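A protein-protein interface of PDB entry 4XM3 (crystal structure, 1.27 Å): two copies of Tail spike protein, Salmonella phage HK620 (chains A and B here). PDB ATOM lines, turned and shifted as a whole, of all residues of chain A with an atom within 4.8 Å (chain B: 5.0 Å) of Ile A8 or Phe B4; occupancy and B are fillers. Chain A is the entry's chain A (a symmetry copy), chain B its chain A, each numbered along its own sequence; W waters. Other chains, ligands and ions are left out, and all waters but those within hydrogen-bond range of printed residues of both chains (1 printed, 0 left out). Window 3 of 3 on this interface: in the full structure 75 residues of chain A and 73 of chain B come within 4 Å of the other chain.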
ATOM      1  N   GLN A   3     -23.081  -2.660 -12.462  1.00  0.00           N
ATOM      2  CA  GLN A   3     -24.418  -3.168 -12.563  1.00  0.00           C
ATOM      3  C   GLN A   3     -24.282  -4.299 -13.582  1.00  0.00           C
ATOM      4  O   GLN A   3     -24.963  -5.293 -13.359  1.00  0.00           O
ATOM      5  CB  GLN A   3     -25.462  -2.119 -12.924  1.00  0.00           C
ATOM      6  CG  GLN A   3     -26.010  -1.337 -11.688  1.00  0.00           C
ATOM      7  CD  GLN A   3     -26.615   0.017 -12.058  1.00  0.00           C
ATOM      8  OE1 GLN A   3     -26.143   0.646 -13.019  1.00  0.00           O
ATOM      9  NE2 GLN A   3     -27.658   0.487 -11.297  1.00  0.00           N
ATOM     10  N   PHE A   4     -23.387  -4.160 -14.597  1.00  0.00           N
ATOM     11  CA  PHE A   4     -23.180  -5.261 -15.588  1.00  0.00           C
ATOM     12  C   PHE A   4     -22.709  -6.554 -14.919  1.00  0.00           C
ATOM     13  O   PHE A   4     -23.349  -7.549 -15.091  1.00  0.00           O
ATOM     14  CB  PHE A   4     -22.202  -4.955 -16.725  1.00  0.00           C
ATOM     15  CG  PHE A   4     -22.139  -6.066 -17.762  1.00  0.00           C
ATOM     16  CD1 PHE A   4     -23.309  -6.442 -18.463  1.00  0.00           C
ATOM     17  CD2 PHE A   4     -20.970  -6.799 -17.951  1.00  0.00           C
ATOM     18  CE1 PHE A   4     -23.257  -7.434 -19.384  1.00  0.00           C
ATOM     19  CE2 PHE A   4     -20.914  -7.811 -18.894  1.00  0.00           C
ATOM     20  CZ  PHE A   4     -22.042  -8.133 -19.603  1.00  0.00           C
ATOM     21  N   ARG A   5     -21.620  -6.523 -14.141  1.00  0.00           N
ATOM     22  CA  ARG A   5     -21.199  -7.754 -13.400  1.00  0.00           C
ATOM     23  C   ARG A   5     -22.348  -8.209 -12.524  1.00  0.00           C
ATOM     24  O   ARG A   5     -22.606  -9.408 -12.431  1.00  0.00           O
ATOM     25  CB  ARG A   5     -19.941  -7.546 -12.516  1.00  0.00           C
ATOM     26  CG  ARG A   5     -19.590  -8.750 -11.586  1.00  0.00           C
ATOM     27  CD  ARG A   5     -18.310  -8.585 -10.745  1.00  0.00           C
ATOM     28  NE  ARG A   5     -17.861  -9.807 -10.027  1.00  0.00           N
ATOM     29  CZ  ARG A   5     -16.678  -9.952  -9.392  1.00  0.00           C
ATOM     30  NH1 ARG A   5     -15.772  -8.960  -9.302  1.00  0.00           N
ATOM     31  NH2 ARG A   5     -16.377 -11.123  -8.820  1.00  0.00           N
ATOM     32  N   ALA A   6     -22.977  -7.276 -11.784  1.00  0.00           N
ATOM     33  CA  ALA A   6     -24.138  -7.619 -10.997  1.00  0.00           C
ATOM     34  C   ALA A   6     -25.247  -8.265 -11.826  1.00  0.00           C
ATOM     35  O   ALA A   6     -25.797  -9.285 -11.387  1.00  0.00           O
ATOM     36  CB  ALA A   6     -24.664  -6.384 -10.299  1.00  0.00           C
ATOM     37  N   ILE A   7     -25.549  -7.697 -13.016  1.00  0.00           N
ATOM     38  CA  ILE A   7     -26.654  -8.219 -13.892  1.00  0.00           C
ATOM     39  C   ILE A   7     -26.271  -9.684 -14.205  1.00  0.00           C
ATOM     40  O   ILE A   7     -27.082 -10.634 -14.114  1.00  0.00           O
ATOM     41  CB  ILE A   7     -26.857  -7.309 -15.195  1.00  0.00           C
ATOM     42  CG1 ILE A   7     -27.517  -5.928 -14.862  1.00  0.00           C
ATOM     43  CG2 ILE A   7     -27.611  -8.031 -16.278  1.00  0.00           C
ATOM     44  CD1 ILE A   7     -27.394  -4.733 -15.892  1.00  0.00           C
ATOM     45  N   ILE A   8     -25.004  -9.878 -14.577  1.00  0.00           N
ATOM     46  CA  ILE A   8     -24.574 -11.180 -15.092  1.00  0.00           C
ATOM     47  C   ILE A   8     -24.700 -12.256 -13.997  1.00  0.00           C
ATOM     48  O   ILE A   8     -25.139 -13.378 -14.304  1.00  0.00           O
ATOM     49  CB  ILE A   8     -23.166 -11.132 -15.765  1.00  0.00           C
ATOM     50  CG1 ILE A   8     -23.197 -10.336 -17.100  1.00  0.00           C
ATOM     51  CG2 ILE A   8     -22.588 -12.563 -16.043  1.00  0.00           C
ATOM     52  CD1 ILE A   8     -24.024 -10.888 -18.252  1.00  0.00           C
ATOM     53  N   GLU A   9     -24.351 -11.938 -12.755  1.00  0.00           N
ATOM     54  CA  GLU A   9     -24.459 -12.907 -11.659  1.00  0.00           C
ATOM     55  C   GLU A   9     -25.860 -13.088 -11.099  1.00  0.00           C
ATOM     56  O   GLU A   9     -26.077 -14.049 -10.332  1.00  0.00           O
ATOM     57  CB  GLU A   9     -23.458 -12.581 -10.495  1.00  0.00           C
ATOM     58  CG  GLU A   9     -22.010 -12.482 -10.993  1.00  0.00           C
ATOM     59  CD  GLU A   9     -20.974 -12.515  -9.928  1.00  0.00           C
ATOM     60  OE1 GLU A   9     -20.629 -13.627  -9.444  1.00  0.00           O
ATOM     61  OE2 GLU A   9     -20.477 -11.433  -9.639  1.00  0.00           O
ATOM     62  N   SER A  10     -26.744 -12.133 -11.403  1.00  0.00           N
ATOM     63  CA  SER A  10     -28.135 -12.160 -10.978  1.00  0.00           C
ATOM     64  C   SER A  10     -28.919 -13.250 -11.733  1.00  0.00           C
ATOM     65  O   SER A  10     -28.444 -13.730 -12.757  1.00  0.00           O
ATOM     66  CB  SER A  10     -28.799 -10.790 -11.207  1.00  0.00           C
ATOM     67  OG  SER A  10     -29.216 -10.592 -12.567  1.00  0.00           O
ATOM     68  N   GLY A  13     -29.080 -12.847 -15.498  1.00  0.00           N
ATOM     69  CA  GLY A  13     -27.827 -12.863 -16.269  1.00  0.00           C
ATOM     70  C   GLY A  13     -27.828 -13.508 -17.613  1.00  0.00           C
ATOM     71  O   GLY A  13     -27.364 -12.931 -18.573  1.00  0.00           O
ATOM     72  N   HIS A  16     -28.963 -11.695 -20.594  1.00  0.00           N
ATOM     73  CA  HIS A  16     -28.136 -10.628 -21.146  1.00  0.00           C
ATOM     74  C   HIS A  16     -26.996 -11.160 -22.013  1.00  0.00           C
ATOM     75  O   HIS A  16     -26.236 -10.368 -22.592  1.00  0.00           O
ATOM     76  CB  HIS A  16     -27.606  -9.757 -19.980  1.00  0.00           C
ATOM     77  CG  HIS A  16     -28.661  -8.902 -19.376  1.00  0.00           C
ATOM     78  ND1 HIS A  16     -29.566  -9.360 -18.452  1.00  0.00           N
ATOM     79  CD2 HIS A  16     -28.964  -7.605 -19.600  1.00  0.00           C
ATOM     80  CE1 HIS A  16     -30.387  -8.383 -18.117  1.00  0.00           C
ATOM     81  NE2 HIS A  16     -30.074  -7.314 -18.840  1.00  0.00           N
ATOM     82  N   VAL A  17     -26.811 -12.500 -22.023  1.00  0.00           N
ATOM     83  CA  VAL A  17     -25.755 -13.062 -22.823  1.00  0.00           C
ATOM     84  C   VAL A  17     -26.271 -13.486 -24.209  1.00  0.00           C
ATOM     85  O   VAL A  17     -27.080 -14.349 -24.310  1.00  0.00           O
ATOM     86  CB  VAL A  17     -25.119 -14.289 -22.158  1.00  0.00           C
ATOM     87  CG1 VAL A  17     -24.003 -14.902 -23.013  1.00  0.00           C
ATOM     88  CG2 VAL A  17     -24.602 -13.936 -20.723  1.00  0.00           C
ATOM     89  N   PRO B   1     -12.353  -7.041 -10.894  1.00  0.00           N
ATOM     90  CA  PRO B   1     -13.083  -7.191 -12.188  1.00  0.00           C
ATOM     91  C   PRO B   1     -12.196  -7.823 -13.283  1.00  0.00           C
ATOM     92  O   PRO B   1     -12.703  -8.253 -14.340  1.00  0.00           O
ATOM     93  CB  PRO B   1     -13.472  -5.730 -12.539  1.00  0.00           C
ATOM     94  CG  PRO B   1     -12.985  -4.865 -11.396  1.00  0.00           C
ATOM     95  CD  PRO B   1     -11.935  -5.648 -10.649  1.00  0.00           C
ATOM     96  N   ASP B   2     -10.882  -7.912 -13.053  1.00  0.00           N
ATOM     97  CA  ASP B   2     -10.061  -8.705 -13.971  1.00  0.00           C
ATOM     98  C   ASP B   2     -10.379 -10.155 -13.865  1.00  0.00           C
ATOM     99  O   ASP B   2     -10.436 -10.849 -14.902  1.00  0.00           O
ATOM    100  CB  ASP B   2      -8.549  -8.446 -13.792  1.00  0.00           C
ATOM    101  CG  ASP B   2      -8.197  -7.055 -14.194  1.00  0.00           C
ATOM    102  OD1 ASP B   2      -8.567  -6.729 -15.357  1.00  0.00           O
ATOM    103  OD2 ASP B   2      -7.630  -6.310 -13.351  1.00  0.00           O
ATOM    104  N   GLN B   3     -10.599 -10.573 -12.618  1.00  0.00           N
ATOM    105  CA  GLN B   3     -10.774 -11.957 -12.287  1.00  0.00           C
ATOM    106  C   GLN B   3     -12.179 -12.262 -12.809  1.00  0.00           C
ATOM    107  O   GLN B   3     -12.324 -13.369 -13.313  1.00  0.00           O
ATOM    108  CB  GLN B   3     -10.568 -12.280 -10.814  1.00  0.00           C
ATOM    109  CG  GLN B   3      -9.074 -12.532 -10.435  1.00  0.00           C
ATOM    110  CD  GLN B   3      -8.790 -12.327  -8.947  1.00  0.00           C
ATOM    111  OE1 GLN B   3      -9.444 -11.477  -8.321  1.00  0.00           O
ATOM    112  NE2 GLN B   3      -7.808 -13.092  -8.367  1.00  0.00           N
ATOM    113  N   PHE B   4     -13.124 -11.285 -12.749  1.00  0.00           N
ATOM    114  CA  PHE B   4     -14.497 -11.518 -13.294  1.00  0.00           C
ATOM    115  C   PHE B   4     -14.471 -11.849 -14.788  1.00  0.00           C
ATOM    116  O   PHE B   4     -14.980 -12.867 -15.154  1.00  0.00           O
ATOM    117  CB  PHE B   4     -15.491 -10.372 -13.099  1.00  0.00           C
ATOM    118  CG  PHE B   4     -16.897 -10.726 -13.562  1.00  0.00           C
ATOM    119  CD1 PHE B   4     -17.576 -11.818 -12.973  1.00  0.00           C
ATOM    120  CD2 PHE B   4     -17.482 -10.063 -14.637  1.00  0.00           C
ATOM    121  CE1 PHE B   4     -18.826 -12.140 -13.386  1.00  0.00           C
ATOM    122  CE2 PHE B   4     -18.761 -10.386 -15.058  1.00  0.00           C
ATOM    123  CZ  PHE B   4     -19.430 -11.415 -14.446  1.00  0.00           C
ATOM    124  N   ARG B   5     -13.858 -11.007 -15.628  1.00  0.00           N
ATOM    125  CA  ARG B   5     -13.737 -11.360 -17.079  1.00  0.00           C
ATOM    126  C   ARG B   5     -13.024 -12.692 -17.196  1.00  0.00           C
ATOM    127  O   ARG B   5     -13.413 -13.521 -18.017  1.00  0.00           O
ATOM    128  CB  ARG B   5     -12.970 -10.301 -17.913  1.00  0.00           C
ATOM    129  CG  ARG B   5     -12.660 -10.726 -19.383  1.00  0.00           C
ATOM    130  CD  ARG B   5     -11.952  -9.664 -20.244  1.00  0.00           C
ATOM    131  NE  ARG B   5     -11.851  -9.985 -21.693  1.00  0.00           N
ATOM    132  CZ  ARG B   5     -11.448  -9.131 -22.658  1.00  0.00           C
ATOM    133  NH1 ARG B   5     -11.041  -7.874 -22.396  1.00  0.00           N
ATOM    134  NH2 ARG B   5     -11.444  -9.534 -23.933  1.00  0.00           N
ATOM    135  N   ALA B   6     -11.908 -12.869 -16.463  1.00  0.00           N
ATOM    136  CA  ALA B   6     -11.229 -14.143 -16.453  1.00  0.00           C
ATOM    137  C   ALA B   6     -12.142 -15.301 -16.051  1.00  0.00           C
ATOM    138  O   ALA B   6     -12.115 -16.338 -16.727  1.00  0.00           O
ATOM    139  CB  ALA B   6     -10.034 -14.077 -15.526  1.00  0.00           C
ATOM    140  N   ILE B   7     -12.954 -15.112 -14.985  1.00  0.00           N
ATOM    141  CA  ILE B   7     -13.859 -16.198 -14.472  1.00  0.00           C
ATOM    142  C   ILE B   7     -14.786 -16.554 -15.657  1.00  0.00           C
ATOM    143  O   ILE B   7     -15.021 -17.734 -16.007  1.00  0.00           O
ATOM    144  CB  ILE B   7     -14.643 -15.740 -13.151  1.00  0.00           C
ATOM    145  CG1 ILE B   7     -13.706 -15.667 -11.898  1.00  0.00           C
ATOM    146  CG2 ILE B   7     -15.851 -16.595 -12.884  1.00  0.00           C
ATOM    147  CD1 ILE B   7     -14.156 -14.825 -10.634  1.00  0.00           C
ATOM    148  N   ILE B   8     -15.323 -15.514 -16.298  1.00  0.00           N
ATOM    149  CA  ILE B   8     -16.370 -15.720 -17.301  1.00  0.00           C
ATOM    150  C   ILE B   8     -15.813 -16.514 -18.499  1.00  0.00           C
ATOM    151  O   ILE B   8     -16.513 -17.405 -19.008  1.00  0.00           O
ATOM    152  CB  ILE B   8     -17.092 -14.398 -17.708  1.00  0.00           C
ATOM    153  CG1 ILE B   8     -17.967 -13.845 -16.548  1.00  0.00           C
ATOM    154  CG2 ILE B   8     -17.991 -14.575 -18.980  1.00  0.00           C
ATOM    155  CD1 ILE B   8     -19.160 -14.669 -16.086  1.00  0.00           C
ATOM    156  N   HIS B  16     -21.148 -18.979 -13.257  1.00  0.00           N
ATOM    157  CA  HIS B  16     -21.283 -17.664 -12.641  1.00  0.00           C
ATOM    158  C   HIS B  16     -22.397 -16.831 -13.277  1.00  0.00           C
ATOM    159  O   HIS B  16     -22.665 -15.707 -12.824  1.00  0.00           O
ATOM    160  CB  HIS B  16     -19.917 -16.938 -12.714  1.00  0.00           C
ATOM    161  CG  HIS B  16     -18.917 -17.501 -11.770  1.00  0.00           C
ATOM    162  ND1 HIS B  16     -18.185 -18.631 -12.033  1.00  0.00           N
ATOM    163  CD2 HIS B  16     -18.553 -17.086 -10.538  1.00  0.00           C
ATOM    164  CE1 HIS B  16     -17.399 -18.895 -11.007  1.00  0.00           C
ATOM    165  NE2 HIS B  16     -17.640 -17.997 -10.058  1.00  0.00           N
ATOM    166  N   VAL B  17     -22.979 -17.338 -14.387  1.00  0.00           N
ATOM    167  CA  VAL B  17     -24.036 -16.601 -15.029  1.00  0.00           C
ATOM    168  C   VAL B  17     -25.417 -17.063 -14.534  1.00  0.00           C
ATOM    169  O   VAL B  17     -25.790 -18.171 -14.741  1.00  0.00           O
ATOM    170  CB  VAL B  17     -24.002 -16.758 -16.555  1.00  0.00           C
ATOM    171  CG1 VAL B  17     -25.136 -15.988 -17.244  1.00  0.00           C
ATOM    172  CG2 VAL B  17     -22.607 -16.337 -17.125  1.00  0.00           C
ATOM    173  N   GLY B  18     -26.167 -16.163 -13.901  1.00  0.00           N
ATOM    174  CA  GLY B  18     -27.437 -16.562 -13.257  1.00  0.00           C
ATOM    175  C   GLY B  18     -28.541 -16.865 -14.283  1.00  0.00           C
ATOM    176  O   GLY B  18     -28.563 -16.290 -15.380  1.00  0.00           O
HETATM  177  O   HOH W   1     -22.276 -15.809 -10.046  1.00  0.00           O
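Water W1 lies within hydrogen-bond range of OE1 of Glu A9 (2.8 Å) and O of His B16 (2.8 Å).
Among the printed residues, merely in contact across the chains: Ser A10 with Gly B18, Ile A8 with Val B17, Glu A9 with His B16, Arg A5 with Phe B4, Gly A13 with Val B17, Ile A8 with His B16, Ile A8 with Phe B4 and Glu A9 with Phe B4.
Arg A5 touches Phe B4, but with the chains exchanged Phe A4 does not touch Arg B5 (8.2 Å). Ile A8 touches Phe B4, but with the chains exchanged Phe A4 does not touch Ile B8 (7.1 Å). Ile A8 touches His B16, but with the chains exchanged His A16 does not touch Ile B8 (9.9 Å). Ile A8 touches Val B17, but with the chains exchanged Val A17 does not touch Ile B8 (6.9 Å). Positions printed for both chains: 3, 4, 5, 6, 7, 8, 16 and 17. Of the 10 pairs that touch across the chains among the printed residues, none has its exchanged pair printed and touching as well.
The backbone carbonyl oxygen (O) of Gly B18 sits at hydrogen-bond distance from the backbone NH (N) of Gly A13 (3.5 Å). The backbone NH of Gly B18 sits at hydrogen-bond distance from the backbone carbonyl oxygen of Ile A8, 3.0 Å away.
The side-chain hydroxyl (OG) of Ser A10 is in hydrogen-bond range of the backbone carbonyl oxygen (O) of Ile A7 (2.6 Å). The backbone carbonyl oxygen (O) of Ile A7 sits close to the backbone NH (N) of Gly A13 (3.3 Å). NE of Arg A5 lies within salt-bridge range of OE2 of Glu A9, at 3.1 Å.
Of chain B, only Phe B4 (3.7 Å), His B16 (3.7 Å), Val B17 (3.5 Å) and Gly B18 (3.0 Å) come within 4 Å of Ile A8. Of the printed residues of chain A, Phe B4 touches Arg A5 (3.6 Å), Ile A8 (3.7 Å) and Glu A9 (3.998 Å). Of the printed residues of chain A, Gly B18 touches Ile A8 (3.0 Å), Ser A10 (3.0 Å) and Gly A13 (3.5 Å). Printed residues of chain B within 4 Å of Glu A9: Phe B4 and His B16. Gln A3 touches none of the printed residues of chain B. The nearest residue of chain B that does not touch Ile A8 is Ile B8 (4.02 Å). The nearest printed residue of chain B that does not touch Arg A5 is Pro B1 (4.2 Å).
Hydrophobic or aromatic side chains of chain B within 4 Å of the printed part of chain A: Phe B4 and Val B17. Printed residues of chain A that touch a printed residue of chain B: Arg A5, Ile A8, Glu A9, Ser A10 and Gly A13.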
